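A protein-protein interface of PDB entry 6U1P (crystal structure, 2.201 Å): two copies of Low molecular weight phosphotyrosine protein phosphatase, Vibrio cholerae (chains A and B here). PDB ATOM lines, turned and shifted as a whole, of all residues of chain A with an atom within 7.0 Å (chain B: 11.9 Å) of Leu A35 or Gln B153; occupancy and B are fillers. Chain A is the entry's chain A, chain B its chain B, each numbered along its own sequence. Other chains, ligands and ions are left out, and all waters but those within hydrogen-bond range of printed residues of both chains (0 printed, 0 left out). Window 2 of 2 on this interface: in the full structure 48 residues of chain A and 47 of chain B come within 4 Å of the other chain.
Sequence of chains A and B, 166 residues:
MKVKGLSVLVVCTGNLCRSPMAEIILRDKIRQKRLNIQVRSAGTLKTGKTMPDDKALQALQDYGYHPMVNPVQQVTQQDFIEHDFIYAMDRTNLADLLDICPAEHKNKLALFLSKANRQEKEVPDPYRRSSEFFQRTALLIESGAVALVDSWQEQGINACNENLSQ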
ATOM      1  N   LYS A  29     -25.641 -33.532   0.145  1.00  0.00           N
ATOM      2  CA  LYS A  29     -25.541 -32.669  -1.027  1.00  0.00           C
ATOM      3  C   LYS A  29     -26.147 -31.296  -0.780  1.00  0.00           C
ATOM      4  O   LYS A  29     -25.658 -30.297  -1.326  1.00  0.00           O
ATOM      5  CB  LYS A  29     -26.209 -33.347  -2.226  1.00  0.00           C
ATOM      6  CG  LYS A  29     -25.643 -34.743  -2.471  1.00  0.00           C
ATOM      7  CD  LYS A  29     -25.151 -34.905  -3.873  1.00  0.00           C
ATOM      8  CE  LYS A  29     -24.114 -36.032  -4.010  1.00  0.00           C
ATOM      9  NZ  LYS A  29     -22.994 -35.995  -3.033  1.00  0.00           N
ATOM     10  N   ILE A  30     -27.206 -31.220   0.028  1.00  0.00           N
ATOM     11  CA  ILE A  30     -27.773 -29.925   0.377  1.00  0.00           C
ATOM     12  C   ILE A  30     -26.776 -29.102   1.192  1.00  0.00           C
ATOM     13  O   ILE A  30     -26.580 -27.907   0.945  1.00  0.00           O
ATOM     14  CB  ILE A  30     -29.096 -30.115   1.134  1.00  0.00           C
ATOM     15  CG1 ILE A  30     -30.190 -30.657   0.213  1.00  0.00           C
ATOM     16  CG2 ILE A  30     -29.533 -28.815   1.793  1.00  0.00           C
ATOM     17  CD1 ILE A  30     -31.338 -31.234   0.995  1.00  0.00           C
ATOM     18  N   ARG A  31     -26.109 -29.735   2.159  1.00  0.00           N
ATOM     19  CA  ARG A  31     -25.188 -28.976   2.994  1.00  0.00           C
ATOM     20  C   ARG A  31     -23.916 -28.621   2.229  1.00  0.00           C
ATOM     21  O   ARG A  31     -23.346 -27.553   2.450  1.00  0.00           O
ATOM     22  CB  ARG A  31     -24.888 -29.750   4.282  1.00  0.00           C
ATOM     23  CG  ARG A  31     -26.175 -30.268   4.996  1.00  0.00           C
ATOM     24  CD  ARG A  31     -26.076 -30.268   6.538  1.00  0.00           C
ATOM     25  NE  ARG A  31     -27.289 -30.746   7.214  1.00  0.00           N
ATOM     26  CZ  ARG A  31     -28.439 -30.076   7.295  1.00  0.00           C
ATOM     27  NH1 ARG A  31     -28.562 -28.872   6.742  1.00  0.00           N
ATOM     28  NH2 ARG A  31     -29.474 -30.612   7.940  1.00  0.00           N
ATOM     29  N   GLN A  32     -23.533 -29.442   1.245  1.00  0.00           N
ATOM     30  CA  GLN A  32     -22.372 -29.144   0.410  1.00  0.00           C
ATOM     31  C   GLN A  32     -22.530 -27.805  -0.305  1.00  0.00           C
ATOM     32  O   GLN A  32     -21.544 -27.089  -0.520  1.00  0.00           O
ATOM     33  CB  GLN A  32     -22.204 -30.260  -0.615  1.00  0.00           C
ATOM     34  CG  GLN A  32     -20.805 -30.588  -0.992  1.00  0.00           C
ATOM     35  CD  GLN A  32     -20.147 -31.499   0.005  1.00  0.00           C
ATOM     36  OE1 GLN A  32     -19.603 -31.042   1.013  1.00  0.00           O
ATOM     37  NE2 GLN A  32     -20.198 -32.806  -0.259  1.00  0.00           N
ATOM     38  N   LYS A  33     -23.761 -27.466  -0.709  1.00  0.00           N
ATOM     39  CA  LYS A  33     -24.060 -26.211  -1.387  1.00  0.00           C
ATOM     40  C   LYS A  33     -24.708 -25.177  -0.465  1.00  0.00           C
ATOM     41  O   LYS A  33     -25.074 -24.091  -0.931  1.00  0.00           O
ATOM     42  CB  LYS A  33     -24.935 -26.474  -2.611  1.00  0.00           C
ATOM     43  CG  LYS A  33     -24.272 -27.399  -3.671  1.00  0.00           C
ATOM     44  CD  LYS A  33     -25.108 -27.447  -4.951  1.00  0.00           C
ATOM     45  CE  LYS A  33     -24.397 -28.182  -6.096  1.00  0.00           C
ATOM     46  NZ  LYS A  33     -23.019 -27.678  -6.427  1.00  0.00           N
ATOM     47  N   ARG A  34     -24.816 -25.479   0.832  1.00  0.00           N
ATOM     48  CA  ARG A  34     -25.477 -24.623   1.828  1.00  0.00           C
ATOM     49  C   ARG A  34     -26.825 -24.109   1.342  1.00  0.00           C
ATOM     50  O   ARG A  34     -27.157 -22.935   1.502  1.00  0.00           O
ATOM     51  CB  ARG A  34     -24.603 -23.425   2.225  1.00  0.00           C
ATOM     52  CG  ARG A  34     -23.218 -23.741   2.721  1.00  0.00           C
ATOM     53  CD  ARG A  34     -22.276 -22.640   2.285  1.00  0.00           C
ATOM     54  N   LEU A  35     -27.643 -25.016   0.823  1.00  0.00           N
ATOM     55  CA  LEU A  35     -28.995 -24.645   0.433  1.00  0.00           C
ATOM     56  C   LEU A  35     -29.915 -24.687   1.646  1.00  0.00           C
ATOM     57  O   LEU A  35     -29.666 -25.406   2.616  1.00  0.00           O
ATOM     58  CB  LEU A  35     -29.513 -25.595  -0.654  1.00  0.00           C
ATOM     59  CG  LEU A  35     -28.592 -25.625  -1.879  1.00  0.00           C
ATOM     60  CD1 LEU A  35     -28.860 -26.787  -2.830  1.00  0.00           C
ATOM     61  CD2 LEU A  35     -28.681 -24.241  -2.627  1.00  0.00           C
ATOM     62  N   ASN A  36     -30.981 -23.895   1.598  1.00  0.00           N
ATOM     63  CA  ASN A  36     -31.945 -23.873   2.698  1.00  0.00           C
ATOM     64  C   ASN A  36     -33.060 -24.884   2.417  1.00  0.00           C
ATOM     65  O   ASN A  36     -34.204 -24.554   2.098  1.00  0.00           O
ATOM     66  CB  ASN A  36     -32.494 -22.471   2.911  1.00  0.00           C
ATOM     67  CG  ASN A  36     -33.444 -22.408   4.089  1.00  0.00           C
ATOM     68  OD1 ASN A  36     -34.399 -21.632   4.095  1.00  0.00           O
ATOM     69  ND2 ASN A  36     -33.202 -23.258   5.088  1.00  0.00           N
ATOM     70  N   ILE A  37     -32.692 -26.154   2.547  1.00  0.00           N
ATOM     71  CA  ILE A  37     -33.613 -27.253   2.308  1.00  0.00           C
ATOM     72  C   ILE A  37     -33.497 -28.239   3.459  1.00  0.00           C
ATOM     73  O   ILE A  37     -32.387 -28.618   3.845  1.00  0.00           O
ATOM     74  CB  ILE A  37     -33.319 -27.962   0.972  1.00  0.00           C
ATOM     75  CG1 ILE A  37     -33.423 -26.987  -0.213  1.00  0.00           C
ATOM     76  CG2 ILE A  37     -34.238 -29.208   0.806  1.00  0.00           C
ATOM     77  CD1 ILE A  37     -32.945 -27.587  -1.553  1.00  0.00           C
ATOM     78  N   GLN A  38     -34.634 -28.675   3.984  1.00  0.00           N
ATOM     79  CA  GLN A  38     -34.661 -29.740   4.966  1.00  0.00           C
ATOM     80  C   GLN A  38     -35.132 -31.021   4.292  1.00  0.00           C
ATOM     81  O   GLN A  38     -35.894 -30.997   3.319  1.00  0.00           O
ATOM     82  CB  GLN A  38     -35.590 -29.399   6.133  1.00  0.00           C
ATOM     83  CG  GLN A  38     -35.118 -28.204   6.924  1.00  0.00           C
ATOM     84  CD  GLN A  38     -36.171 -27.116   7.008  1.00  0.00           C
ATOM     85  OE1 GLN A  38     -37.111 -27.201   7.813  1.00  0.00           O
ATOM     86  NE2 GLN A  38     -36.026 -26.084   6.169  1.00  0.00           N
ATOM     87  N   SER B 143     -27.231 -40.865  -7.802  1.00  0.00           N
ATOM     88  CA  SER B 143     -27.554 -40.282  -9.097  1.00  0.00           C
ATOM     89  C   SER B 143     -28.891 -39.551  -9.046  1.00  0.00           C
ATOM     90  O   SER B 143     -29.004 -38.410  -9.501  1.00  0.00           O
ATOM     91  CB  SER B 143     -27.586 -41.393 -10.149  1.00  0.00           C
ATOM     92  OG  SER B 143     -28.494 -41.092 -11.194  1.00  0.00           O
ATOM     93  N   GLY B 144     -29.900 -40.165  -8.430  1.00  0.00           N
ATOM     94  CA  GLY B 144     -31.177 -39.487  -8.277  1.00  0.00           C
ATOM     95  C   GLY B 144     -31.080 -38.229  -7.435  1.00  0.00           C
ATOM     96  O   GLY B 144     -31.637 -37.182  -7.794  1.00  0.00           O
ATOM     97  N   ALA B 145     -30.361 -38.308  -6.307  1.00  0.00           N
ATOM     98  CA  ALA B 145     -30.276 -37.163  -5.405  1.00  0.00           C
ATOM     99  C   ALA B 145     -29.694 -35.936  -6.108  1.00  0.00           C
ATOM    100  O   ALA B 145     -30.235 -34.830  -5.978  1.00  0.00           O
ATOM    101  CB  ALA B 145     -29.443 -37.529  -4.172  1.00  0.00           C
ATOM    102  N   VAL B 146     -28.612 -36.125  -6.886  1.00  0.00           N
ATOM    103  CA  VAL B 146     -27.956 -34.995  -7.555  1.00  0.00           C
ATOM    104  C   VAL B 146     -28.930 -34.300  -8.494  1.00  0.00           C
ATOM    105  O   VAL B 146     -28.968 -33.063  -8.577  1.00  0.00           O
ATOM    106  CB  VAL B 146     -26.684 -35.451  -8.301  1.00  0.00           C
ATOM    107  CG1 VAL B 146     -26.220 -34.363  -9.287  1.00  0.00           C
ATOM    108  CG2 VAL B 146     -25.576 -35.771  -7.325  1.00  0.00           C
ATOM    109  N   ALA B 147     -29.719 -35.085  -9.233  1.00  0.00           N
ATOM    110  CA  ALA B 147     -30.704 -34.493 -10.137  1.00  0.00           C
ATOM    111  C   ALA B 147     -31.773 -33.717  -9.369  1.00  0.00           C
ATOM    112  O   ALA B 147     -32.140 -32.598  -9.761  1.00  0.00           O
ATOM    113  CB  ALA B 147     -31.337 -35.575 -11.012  1.00  0.00           C
ATOM    114  N   LEU B 148     -32.290 -34.291  -8.275  1.00  0.00           N
ATOM    115  CA  LEU B 148     -33.284 -33.566  -7.485  1.00  0.00           C
ATOM    116  C   LEU B 148     -32.724 -32.232  -6.993  1.00  0.00           C
ATOM    117  O   LEU B 148     -33.401 -31.201  -7.059  1.00  0.00           O
ATOM    118  CB  LEU B 148     -33.735 -34.402  -6.284  1.00  0.00           C
ATOM    119  CG  LEU B 148     -34.615 -35.636  -6.533  1.00  0.00           C
ATOM    120  CD1 LEU B 148     -35.054 -36.264  -5.201  1.00  0.00           C
ATOM    121  CD2 LEU B 148     -35.820 -35.265  -7.380  1.00  0.00           C
ATOM    122  N   VAL B 149     -31.486 -32.236  -6.497  1.00  0.00           N
ATOM    123  CA  VAL B 149     -30.901 -31.010  -5.977  1.00  0.00           C
ATOM    124  C   VAL B 149     -30.778 -29.977  -7.087  1.00  0.00           C
ATOM    125  O   VAL B 149     -30.992 -28.784  -6.863  1.00  0.00           O
ATOM    126  CB  VAL B 149     -29.559 -31.307  -5.284  1.00  0.00           C
ATOM    127  CG1 VAL B 149     -28.787 -30.042  -5.064  1.00  0.00           C
ATOM    128  CG2 VAL B 149     -29.810 -32.011  -3.927  1.00  0.00           C
ATOM    129  N   ASP B 150     -30.464 -30.417  -8.306  1.00  0.00           N
ATOM    130  CA  ASP B 150     -30.436 -29.485  -9.435  1.00  0.00           C
ATOM    131  C   ASP B 150     -31.818 -28.897  -9.691  1.00  0.00           C
ATOM    132  O   ASP B 150     -31.981 -27.672  -9.799  1.00  0.00           O
ATOM    133  CB  ASP B 150     -29.919 -30.180 -10.689  1.00  0.00           C
ATOM    134  CG  ASP B 150     -28.431 -30.414 -10.647  1.00  0.00           C
ATOM    135  OD1 ASP B 150     -27.757 -29.832  -9.771  1.00  0.00           O
ATOM    136  OD2 ASP B 150     -27.932 -31.179 -11.493  1.00  0.00           O
ATOM    137  N   SER B 151     -32.821 -29.770  -9.831  1.00  0.00           N
ATOM    138  CA  SER B 151     -34.182 -29.327 -10.112  1.00  0.00           C
ATOM    139  C   SER B 151     -34.685 -28.342  -9.065  1.00  0.00           C
ATOM    140  O   SER B 151     -35.411 -27.395  -9.392  1.00  0.00           O
ATOM    141  CB  SER B 151     -35.117 -30.530 -10.188  1.00  0.00           C
ATOM    142  OG  SER B 151     -36.415 -30.198  -9.723  1.00  0.00           O
ATOM    143  N   TRP B 152     -34.315 -28.560  -7.800  1.00  0.00           N
ATOM    144  CA  TRP B 152     -34.762 -27.688  -6.718  1.00  0.00           C
ATOM    145  C   TRP B 152     -34.212 -26.280  -6.875  1.00  0.00           C
ATOM    146  O   TRP B 152     -34.904 -25.294  -6.576  1.00  0.00           O
ATOM    147  CB  TRP B 152     -34.363 -28.274  -5.366  1.00  0.00           C
ATOM    148  CG  TRP B 152     -35.055 -29.541  -5.080  1.00  0.00           C
ATOM    149  CD1 TRP B 152     -36.197 -29.989  -5.666  1.00  0.00           C
ATOM    150  CD2 TRP B 152     -34.665 -30.539  -4.133  1.00  0.00           C
ATOM    151  NE1 TRP B 152     -36.551 -31.206  -5.140  1.00  0.00           N
ATOM    152  CE2 TRP B 152     -35.624 -31.572  -4.200  1.00  0.00           C
ATOM    153  CE3 TRP B 152     -33.599 -30.662  -3.236  1.00  0.00           C
ATOM    154  CZ2 TRP B 152     -35.545 -32.727  -3.404  1.00  0.00           C
ATOM    155  CZ3 TRP B 152     -33.520 -31.807  -2.447  1.00  0.00           C
ATOM    156  CH2 TRP B 152     -34.494 -32.821  -2.534  1.00  0.00           C
ATOM    157  N   GLN B 153     -32.983 -26.154  -7.368  1.00  0.00           N
ATOM    158  CA  GLN B 153     -32.537 -24.778  -7.491  1.00  0.00           C
ATOM    159  C   GLN B 153     -33.144 -24.099  -8.710  1.00  0.00           C
ATOM    160  O   GLN B 153     -32.822 -22.938  -8.975  1.00  0.00           O
ATOM    161  CB  GLN B 153     -31.007 -24.730  -7.521  1.00  0.00           C
ATOM    162  CG  GLN B 153     -30.365 -25.590  -6.433  1.00  0.00           C
ATOM    163  CD  GLN B 153     -28.854 -25.721  -6.587  1.00  0.00           C
ATOM    164  OE1 GLN B 153     -28.134 -24.742  -6.485  1.00  0.00           O
ATOM    165  NE2 GLN B 153     -28.373 -26.942  -6.832  1.00  0.00           N
ATOM    166  N   GLU B 154     -34.041 -24.793  -9.417  1.00  0.00           N
ATOM    167  CA  GLU B 154     -34.760 -24.270 -10.578  1.00  0.00           C
ATOM    168  C   GLU B 154     -36.265 -24.330 -10.359  1.00  0.00           C
ATOM    169  O   GLU B 154     -36.832 -23.440  -9.740  1.00  0.00           O
ATOM    170  CB  GLU B 154     -34.400 -25.052 -11.844  1.00  0.00           C
ATOM    171  CG  GLU B 154     -33.005 -25.618 -11.890  1.00  0.00           C
ATOM    172  CD  GLU B 154     -31.956 -24.633 -11.420  1.00  0.00           C
ATOM    173  OE1 GLU B 154     -31.023 -25.063 -10.725  1.00  0.00           O
ATOM    174  OE2 GLU B 154     -32.087 -23.425 -11.691  1.00  0.00           O
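N of Leu A35 sits at hydrogen-bond distance from O of Ile A30 (3.1 Å).
The backbone carbonyl oxygen of Val B149 is in hydrogen-bond range of the side-chain amide nitrogen of Gln B153 (3.2 Å).
Lys A29 touches Val B146 (CD to CG2, 3.6 Å).
CD of Lys A33 touches NE2 of Gln B153 (3.8 Å).
Leu A35 touches Val B149.
Leu A35 touches Gln B153 (CD1 to CD, 3.9 Å).
Ile A37 touches Trp B152 (CD1 to CE3, 3.6 Å).
Of chain B, only Val B149 and Gln B153 come within 4 Å of Leu A35.
Of chain A, only Lys A33 (3.8 Å) and Leu A35 (3.9 Å) come within 4 Å of Gln B153.
No residue of chain B comes within 4 Å of Ile A30.
No residue of chain B comes within 4 Å of Arg A31.
Lys A33 touches just one residue of chain B: Gln B153.
No residue of chain B comes within 4 Å of Arg A34.
Asn A36 touches none of the printed residues of chain B.
Of the printed residues of chain A, Val B149 touches Leu A35 (3.9 Å).
Of the printed residues of chain A, Trp B152 touches Ile A37.
The nearest printed residue of chain B that does not touch Lys A29 is Val B149 (4.2 Å).
Of the 10 printed residues of chain A, 4 touch a printed residue of chain B.
Along chain A the printed residues that touch a printed residue of chain B span positions 29 to 37.
Among the printed residues, no Asp or Glu carboxylate lies within 4 Å of a Lys or Arg side-chain nitrogen of the other chain.
No position is printed for both chains.
Of the 5 pairs that touch across the chains among the printed residues, none has its exchanged pair printed and touching as well.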
